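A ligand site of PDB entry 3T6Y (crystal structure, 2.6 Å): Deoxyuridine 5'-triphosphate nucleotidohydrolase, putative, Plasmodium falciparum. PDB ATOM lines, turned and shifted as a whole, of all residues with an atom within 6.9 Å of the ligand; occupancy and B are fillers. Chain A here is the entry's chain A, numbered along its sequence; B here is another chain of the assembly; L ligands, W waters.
Water W2 lies within hydrogen-bond range of the backbone NH (N) of Ala 119 (2.7 Å), the side-chain amide oxygen (OD1) of Asn 103 (3.0 Å) and an oxygen (O2) of the ligand (3.0 Å).
Water W3 bridges OD2 of Asp 109 and O4 of the ligand.
Water W1 lies within hydrogen-bond range of N of Leu 107 (2.9 Å) and ND2 of Asn 103 (3.3 Å).
The side-chain hydroxyl (OG) of Ser 95 of chain B is in hydrogen-bond range of the backbone carbonyl oxygen (O) of Ser 92 of chain B.
The backbone carbonyl oxygen of Gly 106 lies within hydrogen-bond range of the backbone NH of Leu 88 (2.8 Å).
OH of Tyr 112 sits at hydrogen-bond distance from O of Glu 115, 3.2 Å away.
The backbone carbonyl oxygen (O) of Ala 119 is in hydrogen-bond range of the backbone NH (N) of Ala 102 (2.9 Å).
Phe 46 touches the ligand.
Leu 88 touches the ligand.
Gly 106 touches the ligand.
Leu 107 touches the ligand.
Ile 108 touches the ligand.
CA of Ile 116 touches O1 of the ligand, at 3.6 Å.
CB of Ala 119 touches C11 of the ligand, at 3.8 Å.
Ser 92 of chain B touches the ligand (O to C12, 3.0 Å).
Ser 95 of chain B touches the ligand.
Hydrophobic or aromatic side chains within 4 Å of the ligand: Phe 46, Leu 88, Ile 108, Tyr 112, Ile 117 and Ala 119.
The nearest printed residue that does not touch the ligand is Glu 115 (4.04 Å).
The backbone NH (N) of Ile 117 sits at hydrogen-bond distance from an oxygen (O1) of the ligand (2.9 Å).
A nitrogen (N2) of the ligand is in hydrogen-bond range of the backbone carbonyl oxygen (O) of Ile 117.
The side-chain amide nitrogen (ND2) of Asn 103 is in hydrogen-bond range of an oxygen (O2) of the ligand, at 3.2 Å.
O3 of the ligand sits at hydrogen-bond distance from OH of Tyr 112 (3.3 Å).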
ATOM      1  N   PHE A  46      -6.525   3.539 -14.862  1.00  0.00           N
ATOM      2  CA  PHE A  46      -6.084   3.996 -13.559  1.00  0.00           C
ATOM      3  C   PHE A  46      -6.957   3.382 -12.475  1.00  0.00           C
ATOM      4  O   PHE A  46      -8.041   3.873 -12.173  1.00  0.00           O
ATOM      5  CB  PHE A  46      -6.035   5.517 -13.482  1.00  0.00           C
ATOM      6  CG  PHE A  46      -5.094   6.092 -14.489  1.00  0.00           C
ATOM      7  CD1 PHE A  46      -3.725   6.179 -14.218  1.00  0.00           C
ATOM      8  CD2 PHE A  46      -5.538   6.468 -15.750  1.00  0.00           C
ATOM      9  CE1 PHE A  46      -2.827   6.688 -15.157  1.00  0.00           C
ATOM     10  CE2 PHE A  46      -4.656   6.981 -16.704  1.00  0.00           C
ATOM     11  CZ  PHE A  46      -3.295   7.083 -16.409  1.00  0.00           C
ATOM     12  N   LEU A  88       5.582   1.994  -4.949  1.00  0.00           N
ATOM     13  CA  LEU A  88       4.554   1.068  -5.346  1.00  0.00           C
ATOM     14  C   LEU A  88       5.163   0.184  -6.442  1.00  0.00           C
ATOM     15  O   LEU A  88       5.462   0.679  -7.552  1.00  0.00           O
ATOM     16  CB  LEU A  88       3.352   1.854  -5.833  1.00  0.00           C
ATOM     17  CG  LEU A  88       2.178   1.026  -6.324  1.00  0.00           C
ATOM     18  CD1 LEU A  88       1.220   0.665  -5.196  1.00  0.00           C
ATOM     19  CD2 LEU A  88       1.406   1.732  -7.401  1.00  0.00           C
ATOM     20  N   LEU A 101       2.801  -2.247 -15.311  1.00  0.00           N
ATOM     21  CA  LEU A 101       2.628  -1.006 -14.577  1.00  0.00           C
ATOM     22  C   LEU A 101       3.213   0.134 -15.435  1.00  0.00           C
ATOM     23  O   LEU A 101       4.416   0.203 -15.695  1.00  0.00           O
ATOM     24  CB  LEU A 101       3.244  -1.110 -13.170  1.00  0.00           C
ATOM     25  CG  LEU A 101       2.812  -0.098 -12.084  1.00  0.00           C
ATOM     26  CD1 LEU A 101       1.407  -0.380 -11.631  1.00  0.00           C
ATOM     27  CD2 LEU A 101       3.690  -0.135 -10.855  1.00  0.00           C
ATOM     28  N   ALA A 102       2.353   1.022 -15.894  1.00  0.00           N
ATOM     29  CA  ALA A 102       2.738   2.040 -16.872  1.00  0.00           C
ATOM     30  C   ALA A 102       3.921   2.938 -16.466  1.00  0.00           C
ATOM     31  O   ALA A 102       4.767   3.212 -17.334  1.00  0.00           O
ATOM     32  CB  ALA A 102       1.522   2.872 -17.255  1.00  0.00           C
ATOM     33  N   ASN A 103       3.982   3.390 -15.195  1.00  0.00           N
ATOM     34  CA  ASN A 103       5.119   4.155 -14.700  1.00  0.00           C
ATOM     35  C   ASN A 103       6.227   3.334 -14.026  1.00  0.00           C
ATOM     36  O   ASN A 103       7.024   3.880 -13.230  1.00  0.00           O
ATOM     37  CB  ASN A 103       4.676   5.286 -13.785  1.00  0.00           C
ATOM     38  CG  ASN A 103       3.839   4.807 -12.615  1.00  0.00           C
ATOM     39  OD1 ASN A 103       3.008   3.905 -12.754  1.00  0.00           O
ATOM     40  ND2 ASN A 103       4.019   5.449 -11.455  1.00  0.00           N
ATOM     41  N   ILE A 105       7.654   1.942 -11.529  1.00  0.00           N
ATOM     42  CA  ILE A 105       7.551   1.859 -10.048  1.00  0.00           C
ATOM     43  C   ILE A 105       6.976   3.160  -9.602  1.00  0.00           C
ATOM     44  O   ILE A 105       7.502   4.166  -9.979  1.00  0.00           O
ATOM     45  CB  ILE A 105       8.938   1.735  -9.395  1.00  0.00           C
ATOM     46  CG1 ILE A 105       9.720   0.568  -9.980  1.00  0.00           C
ATOM     47  CG2 ILE A 105       8.820   1.614  -7.896  1.00  0.00           C
ATOM     48  CD1 ILE A 105       9.145  -0.820  -9.675  1.00  0.00           C
ATOM     49  N   GLY A 106       5.882   3.176  -8.866  1.00  0.00           N
ATOM     50  CA  GLY A 106       5.251   4.418  -8.527  1.00  0.00           C
ATOM     51  C   GLY A 106       6.037   4.981  -7.355  1.00  0.00           C
ATOM     52  O   GLY A 106       6.448   4.257  -6.449  1.00  0.00           O
ATOM     53  N   LEU A 107       6.308   6.284  -7.403  1.00  0.00           N
ATOM     54  CA  LEU A 107       6.835   6.994  -6.281  1.00  0.00           C
ATOM     55  C   LEU A 107       5.750   7.769  -5.526  1.00  0.00           C
ATOM     56  O   LEU A 107       5.170   8.695  -6.058  1.00  0.00           O
ATOM     57  CB  LEU A 107       7.908   7.946  -6.748  1.00  0.00           C
ATOM     58  CG  LEU A 107       8.907   8.210  -5.626  1.00  0.00           C
ATOM     59  CD1 LEU A 107      10.281   8.370  -6.221  1.00  0.00           C
ATOM     60  CD2 LEU A 107       8.524   9.429  -4.830  1.00  0.00           C
ATOM     61  N   ILE A 108       5.477   7.431  -4.282  1.00  0.00           N
ATOM     62  CA  ILE A 108       4.464   8.164  -3.560  1.00  0.00           C
ATOM     63  C   ILE A 108       5.267   9.005  -2.569  1.00  0.00           C
ATOM     64  O   ILE A 108       6.036   8.445  -1.794  1.00  0.00           O
ATOM     65  CB  ILE A 108       3.582   7.243  -2.760  1.00  0.00           C
ATOM     66  CG1 ILE A 108       3.083   6.051  -3.613  1.00  0.00           C
ATOM     67  CG2 ILE A 108       2.492   8.050  -2.071  1.00  0.00           C
ATOM     68  CD1 ILE A 108       1.942   6.349  -4.559  1.00  0.00           C
ATOM     69  N   ASP A 109       5.098  10.329  -2.618  1.00  0.00           N
ATOM     70  CA  ASP A 109       5.845  11.309  -1.812  1.00  0.00           C
ATOM     71  C   ASP A 109       5.311  11.413  -0.395  1.00  0.00           C
ATOM     72  O   ASP A 109       4.099  11.118  -0.152  1.00  0.00           O
ATOM     73  CB  ASP A 109       5.798  12.686  -2.479  1.00  0.00           C
ATOM     74  CG  ASP A 109       6.619  12.740  -3.765  1.00  0.00           C
ATOM     75  OD1 ASP A 109       7.880  12.572  -3.697  1.00  0.00           O
ATOM     76  OD2 ASP A 109       5.982  12.948  -4.851  1.00  0.00           O
ATOM     77  N   TYR A 112       1.685  12.899   0.483  1.00  0.00           N
ATOM     78  CA  TYR A 112       0.571  12.623  -0.398  1.00  0.00           C
ATOM     79  C   TYR A 112      -0.629  12.032   0.339  1.00  0.00           C
ATOM     80  O   TYR A 112      -0.505  10.983   1.002  1.00  0.00           O
ATOM     81  CB  TYR A 112       1.025  11.754  -1.572  1.00  0.00           C
ATOM     82  CG  TYR A 112      -0.095  11.422  -2.517  1.00  0.00           C
ATOM     83  CD1 TYR A 112      -0.564  12.367  -3.436  1.00  0.00           C
ATOM     84  CD2 TYR A 112      -0.724  10.174  -2.470  1.00  0.00           C
ATOM     85  CE1 TYR A 112      -1.609  12.077  -4.306  1.00  0.00           C
ATOM     86  CE2 TYR A 112      -1.765   9.873  -3.328  1.00  0.00           C
ATOM     87  CZ  TYR A 112      -2.165  10.840  -4.234  1.00  0.00           C
ATOM     88  OH  TYR A 112      -3.168  10.561  -5.061  1.00  0.00           O
ATOM     89  N   GLY A 114      -3.805  11.425  -1.273  1.00  0.00           N
ATOM     90  CA  GLY A 114      -4.782  10.940  -2.240  1.00  0.00           C
ATOM     91  C   GLY A 114      -4.968   9.418  -2.221  1.00  0.00           C
ATOM     92  O   GLY A 114      -4.210   8.684  -1.561  1.00  0.00           O
ATOM     93  N   GLU A 115      -5.994   8.937  -2.908  1.00  0.00           N
ATOM     94  CA  GLU A 115      -6.176   7.494  -3.045  1.00  0.00           C
ATOM     95  C   GLU A 115      -5.020   6.980  -3.878  1.00  0.00           C
ATOM     96  O   GLU A 115      -4.595   7.671  -4.805  1.00  0.00           O
ATOM     97  CB  GLU A 115      -7.488   7.206  -3.729  1.00  0.00           C
ATOM     98  CG  GLU A 115      -7.836   5.734  -3.889  1.00  0.00           C
ATOM     99  CD  GLU A 115      -9.269   5.574  -4.365  1.00  0.00           C
ATOM    100  OE1 GLU A 115      -9.907   4.494  -4.177  1.00  0.00           O
ATOM    101  OE2 GLU A 115      -9.776   6.579  -4.916  1.00  0.00           O
ATOM    102  N   ILE A 116      -4.476   5.821  -3.513  1.00  0.00           N
ATOM    103  CA  ILE A 116      -3.343   5.191  -4.192  1.00  0.00           C
ATOM    104  C   ILE A 116      -3.867   4.520  -5.458  1.00  0.00           C
ATOM    105  O   ILE A 116      -4.822   3.688  -5.433  1.00  0.00           O
ATOM    106  CB  ILE A 116      -2.746   4.085  -3.321  1.00  0.00           C
ATOM    107  CG1 ILE A 116      -2.506   4.544  -1.847  1.00  0.00           C
ATOM    108  CG2 ILE A 116      -1.533   3.496  -3.976  1.00  0.00           C
ATOM    109  CD1 ILE A 116      -1.269   5.363  -1.550  1.00  0.00           C
ATOM    110  N   ILE A 117      -3.240   4.854  -6.581  1.00  0.00           N
ATOM    111  CA  ILE A 117      -3.691   4.371  -7.847  1.00  0.00           C
ATOM    112  C   ILE A 117      -2.615   3.518  -8.467  1.00  0.00           C
ATOM    113  O   ILE A 117      -1.449   3.918  -8.494  1.00  0.00           O
ATOM    114  CB  ILE A 117      -3.908   5.551  -8.802  1.00  0.00           C
ATOM    115  CG1 ILE A 117      -4.788   6.631  -8.183  1.00  0.00           C
ATOM    116  CG2 ILE A 117      -4.530   5.062 -10.094  1.00  0.00           C
ATOM    117  CD1 ILE A 117      -6.250   6.293  -8.317  1.00  0.00           C
ATOM    118  N   ALA A 118      -3.009   2.380  -9.050  1.00  0.00           N
ATOM    119  CA  ALA A 118      -2.143   1.633  -9.943  1.00  0.00           C
ATOM    120  C   ALA A 118      -2.553   1.893 -11.410  1.00  0.00           C
ATOM    121  O   ALA A 118      -3.718   1.636 -11.796  1.00  0.00           O
ATOM    122  CB  ALA A 118      -2.222   0.150  -9.627  1.00  0.00           C
ATOM    123  N   ALA A 119      -1.617   2.369 -12.207  1.00  0.00           N
ATOM    124  CA  ALA A 119      -1.833   2.624 -13.635  1.00  0.00           C
ATOM    125  C   ALA A 119      -1.417   1.402 -14.413  1.00  0.00           C
ATOM    126  O   ALA A 119      -0.223   1.165 -14.586  1.00  0.00           O
ATOM    127  CB  ALA A 119      -0.999   3.803 -14.102  1.00  0.00           C
ATOM    128  N   ARG B  91       8.187   9.794 -14.488  1.00  0.00           N
ATOM    129  CA  ARG B  91       7.243  10.528 -13.700  1.00  0.00           C
ATOM    130  C   ARG B  91       5.918   9.840 -13.895  1.00  0.00           C
ATOM    131  O   ARG B  91       5.638   9.284 -14.957  1.00  0.00           O
ATOM    132  CB  ARG B  91       7.140  11.973 -14.123  1.00  0.00           C
ATOM    133  CG  ARG B  91       8.406  12.786 -13.889  1.00  0.00           C
ATOM    134  CD  ARG B  91       8.289  14.227 -14.350  1.00  0.00           C
ATOM    135  NE  ARG B  91       7.479  14.965 -13.381  1.00  0.00           N
ATOM    136  CZ  ARG B  91       6.298  15.553 -13.635  1.00  0.00           C
ATOM    137  NH1 ARG B  91       5.766  15.548 -14.848  1.00  0.00           N
ATOM    138  NH2 ARG B  91       5.648  16.157 -12.667  1.00  0.00           N
ATOM    139  N   SER B  92       5.071   9.886 -12.873  1.00  0.00           N
ATOM    140  CA  SER B  92       3.849   9.120 -12.894  1.00  0.00           C
ATOM    141  C   SER B  92       3.030   9.635 -14.071  1.00  0.00           C
ATOM    142  O   SER B  92       2.175   8.952 -14.592  1.00  0.00           O
ATOM    143  CB  SER B  92       3.087   9.275 -11.568  1.00  0.00           C
ATOM    144  OG  SER B  92       2.532  10.570 -11.529  1.00  0.00           O
ATOM    145  N   SER B  93       3.286  10.851 -14.483  1.00  0.00           N
ATOM    146  CA  SER B  93       2.474  11.463 -15.535  1.00  0.00           C
ATOM    147  C   SER B  93       2.751  10.815 -16.937  1.00  0.00           C
ATOM    148  O   SER B  93       1.910  10.937 -17.851  1.00  0.00           O
ATOM    149  CB  SER B  93       2.613  12.989 -15.551  1.00  0.00           C
ATOM    150  OG  SER B  93       3.775  13.381 -16.294  1.00  0.00           O
ATOM    151  N   ILE B  94       3.901  10.116 -17.054  1.00  0.00           N
ATOM    152  CA  ILE B  94       4.301   9.464 -18.277  1.00  0.00           C
ATOM    153  C   ILE B  94       3.223   8.484 -18.641  1.00  0.00           C
ATOM    154  O   ILE B  94       3.111   8.087 -19.788  1.00  0.00           O
ATOM    155  CB  ILE B  94       5.622   8.685 -18.142  1.00  0.00           C
ATOM    156  CG1 ILE B  94       6.154   8.302 -19.529  1.00  0.00           C
ATOM    157  CG2 ILE B  94       5.403   7.400 -17.384  1.00  0.00           C
ATOM    158  CD1 ILE B  94       7.639   8.140 -19.576  1.00  0.00           C
ATOM    159  N   SER B  95       2.407   8.117 -17.683  1.00  0.00           N
ATOM    160  CA  SER B  95       1.456   7.062 -17.936  1.00  0.00           C
ATOM    161  C   SER B  95       0.259   7.545 -18.741  1.00  0.00           C
ATOM    162  O   SER B  95      -0.532   6.728 -19.228  1.00  0.00           O
ATOM    163  CB  SER B  95       1.031   6.419 -16.625  1.00  0.00           C
ATOM    164  OG  SER B  95       0.287   7.352 -15.880  1.00  0.00           O
ATOM    165  N   LYS B  96       0.126   8.858 -18.869  1.00  0.00           N
ATOM    166  CA  LYS B  96      -0.921   9.475 -19.695  1.00  0.00           C
ATOM    167  C   LYS B  96      -0.502   9.434 -21.166  1.00  0.00           C
ATOM    168  O   LYS B  96      -1.341   9.658 -22.013  1.00  0.00           O
ATOM    169  CB  LYS B  96      -1.136  10.946 -19.334  1.00  0.00           C
ATOM    170  CG  LYS B  96      -1.610  11.204 -17.912  1.00  0.00           C
ATOM    171  CD  LYS B  96      -1.708  12.708 -17.620  1.00  0.00           C
ATOM    172  CE  LYS B  96      -1.718  13.011 -16.120  1.00  0.00           C
ATOM    173  NZ  LYS B  96      -1.111  14.350 -15.842  1.00  0.00           N
HETATM  174  N1  LIG L   1       0.682   7.871  -7.206  1.00  0.00           N
HETATM  175  C1  LIG L   1      -0.016   6.720  -7.143  1.00  0.00           C
HETATM  176  O1  LIG L   1      -1.056   6.715  -6.494  1.00  0.00           O
HETATM  177  N2  LIG L   1       0.444   5.597  -7.806  1.00  0.00           N
HETATM  178  C2  LIG L   1       1.654   5.647  -8.523  1.00  0.00           C
HETATM  179  O2  LIG L   1       2.066   4.636  -9.092  1.00  0.00           O
HETATM  180  C3  LIG L   1       2.398   6.818  -8.585  1.00  0.00           C
HETATM  181  C4  LIG L   1       1.908   7.918  -7.908  1.00  0.00           C
HETATM  182  C5  LIG L   1       0.130   9.018  -6.480  1.00  0.00           C
HETATM  183  C6  LIG L   1      -2.484   9.775 -10.847  1.00  0.00           C
HETATM  184  C7  LIG L   1      -1.581   8.843 -11.364  1.00  0.00           C
HETATM  185  C8  LIG L   1      -1.493   7.675 -10.586  1.00  0.00           C
HETATM  186  C9  LIG L   1       1.237  10.012  -6.234  1.00  0.00           C
HETATM  187  C10 LIG L   1      -0.650   6.622 -10.853  1.00  0.00           C
HETATM  188  C11 LIG L   1       0.123   6.716 -11.989  1.00  0.00           C
HETATM  189  C12 LIG L   1       0.025   7.856 -12.789  1.00  0.00           C
HETATM  190  C13 LIG L   1      -0.807   8.937 -12.500  1.00  0.00           C
HETATM  191  C14 LIG L   1      -3.842   9.973 -11.225  1.00  0.00           C
HETATM  192  N3  LIG L   1      -4.635  10.728 -10.439  1.00  0.00           N
HETATM  193  C15 LIG L   1      -5.960  10.999 -11.037  1.00  0.00           C
HETATM  194  C16 LIG L   1      -5.925  10.249 -12.347  1.00  0.00           C
HETATM  195  N4  LIG L   1      -4.574   9.687 -12.348  1.00  0.00           N
HETATM  196  C17 LIG L   1      -4.188   8.989 -13.502  1.00  0.00           C
HETATM  197  C18 LIG L   1       1.101  10.981  -7.363  1.00  0.00           C
HETATM  198  C19 LIG L   1      -0.359  10.947  -7.820  1.00  0.00           C
HETATM  199  O3  LIG L   1      -0.899   9.723  -7.232  1.00  0.00           O
HETATM  200  O4  LIG L   1       1.277  12.153  -6.655  1.00  0.00           O
HETATM  201  C20 LIG L   1      -0.684  10.905  -9.342  1.00  0.00           C
HETATM  202  N5  LIG L   1      -2.074  10.327  -9.503  1.00  0.00           N
HETATM  203  O   HOH W   1       5.317   7.885  -9.670  1.00  0.00           O
HETATM  204  O   HOH W   2       0.792   2.871 -11.096  1.00  0.00           O
HETATM  205  O   HOH W   3       3.479  11.769  -4.590  1.00  0.00           O
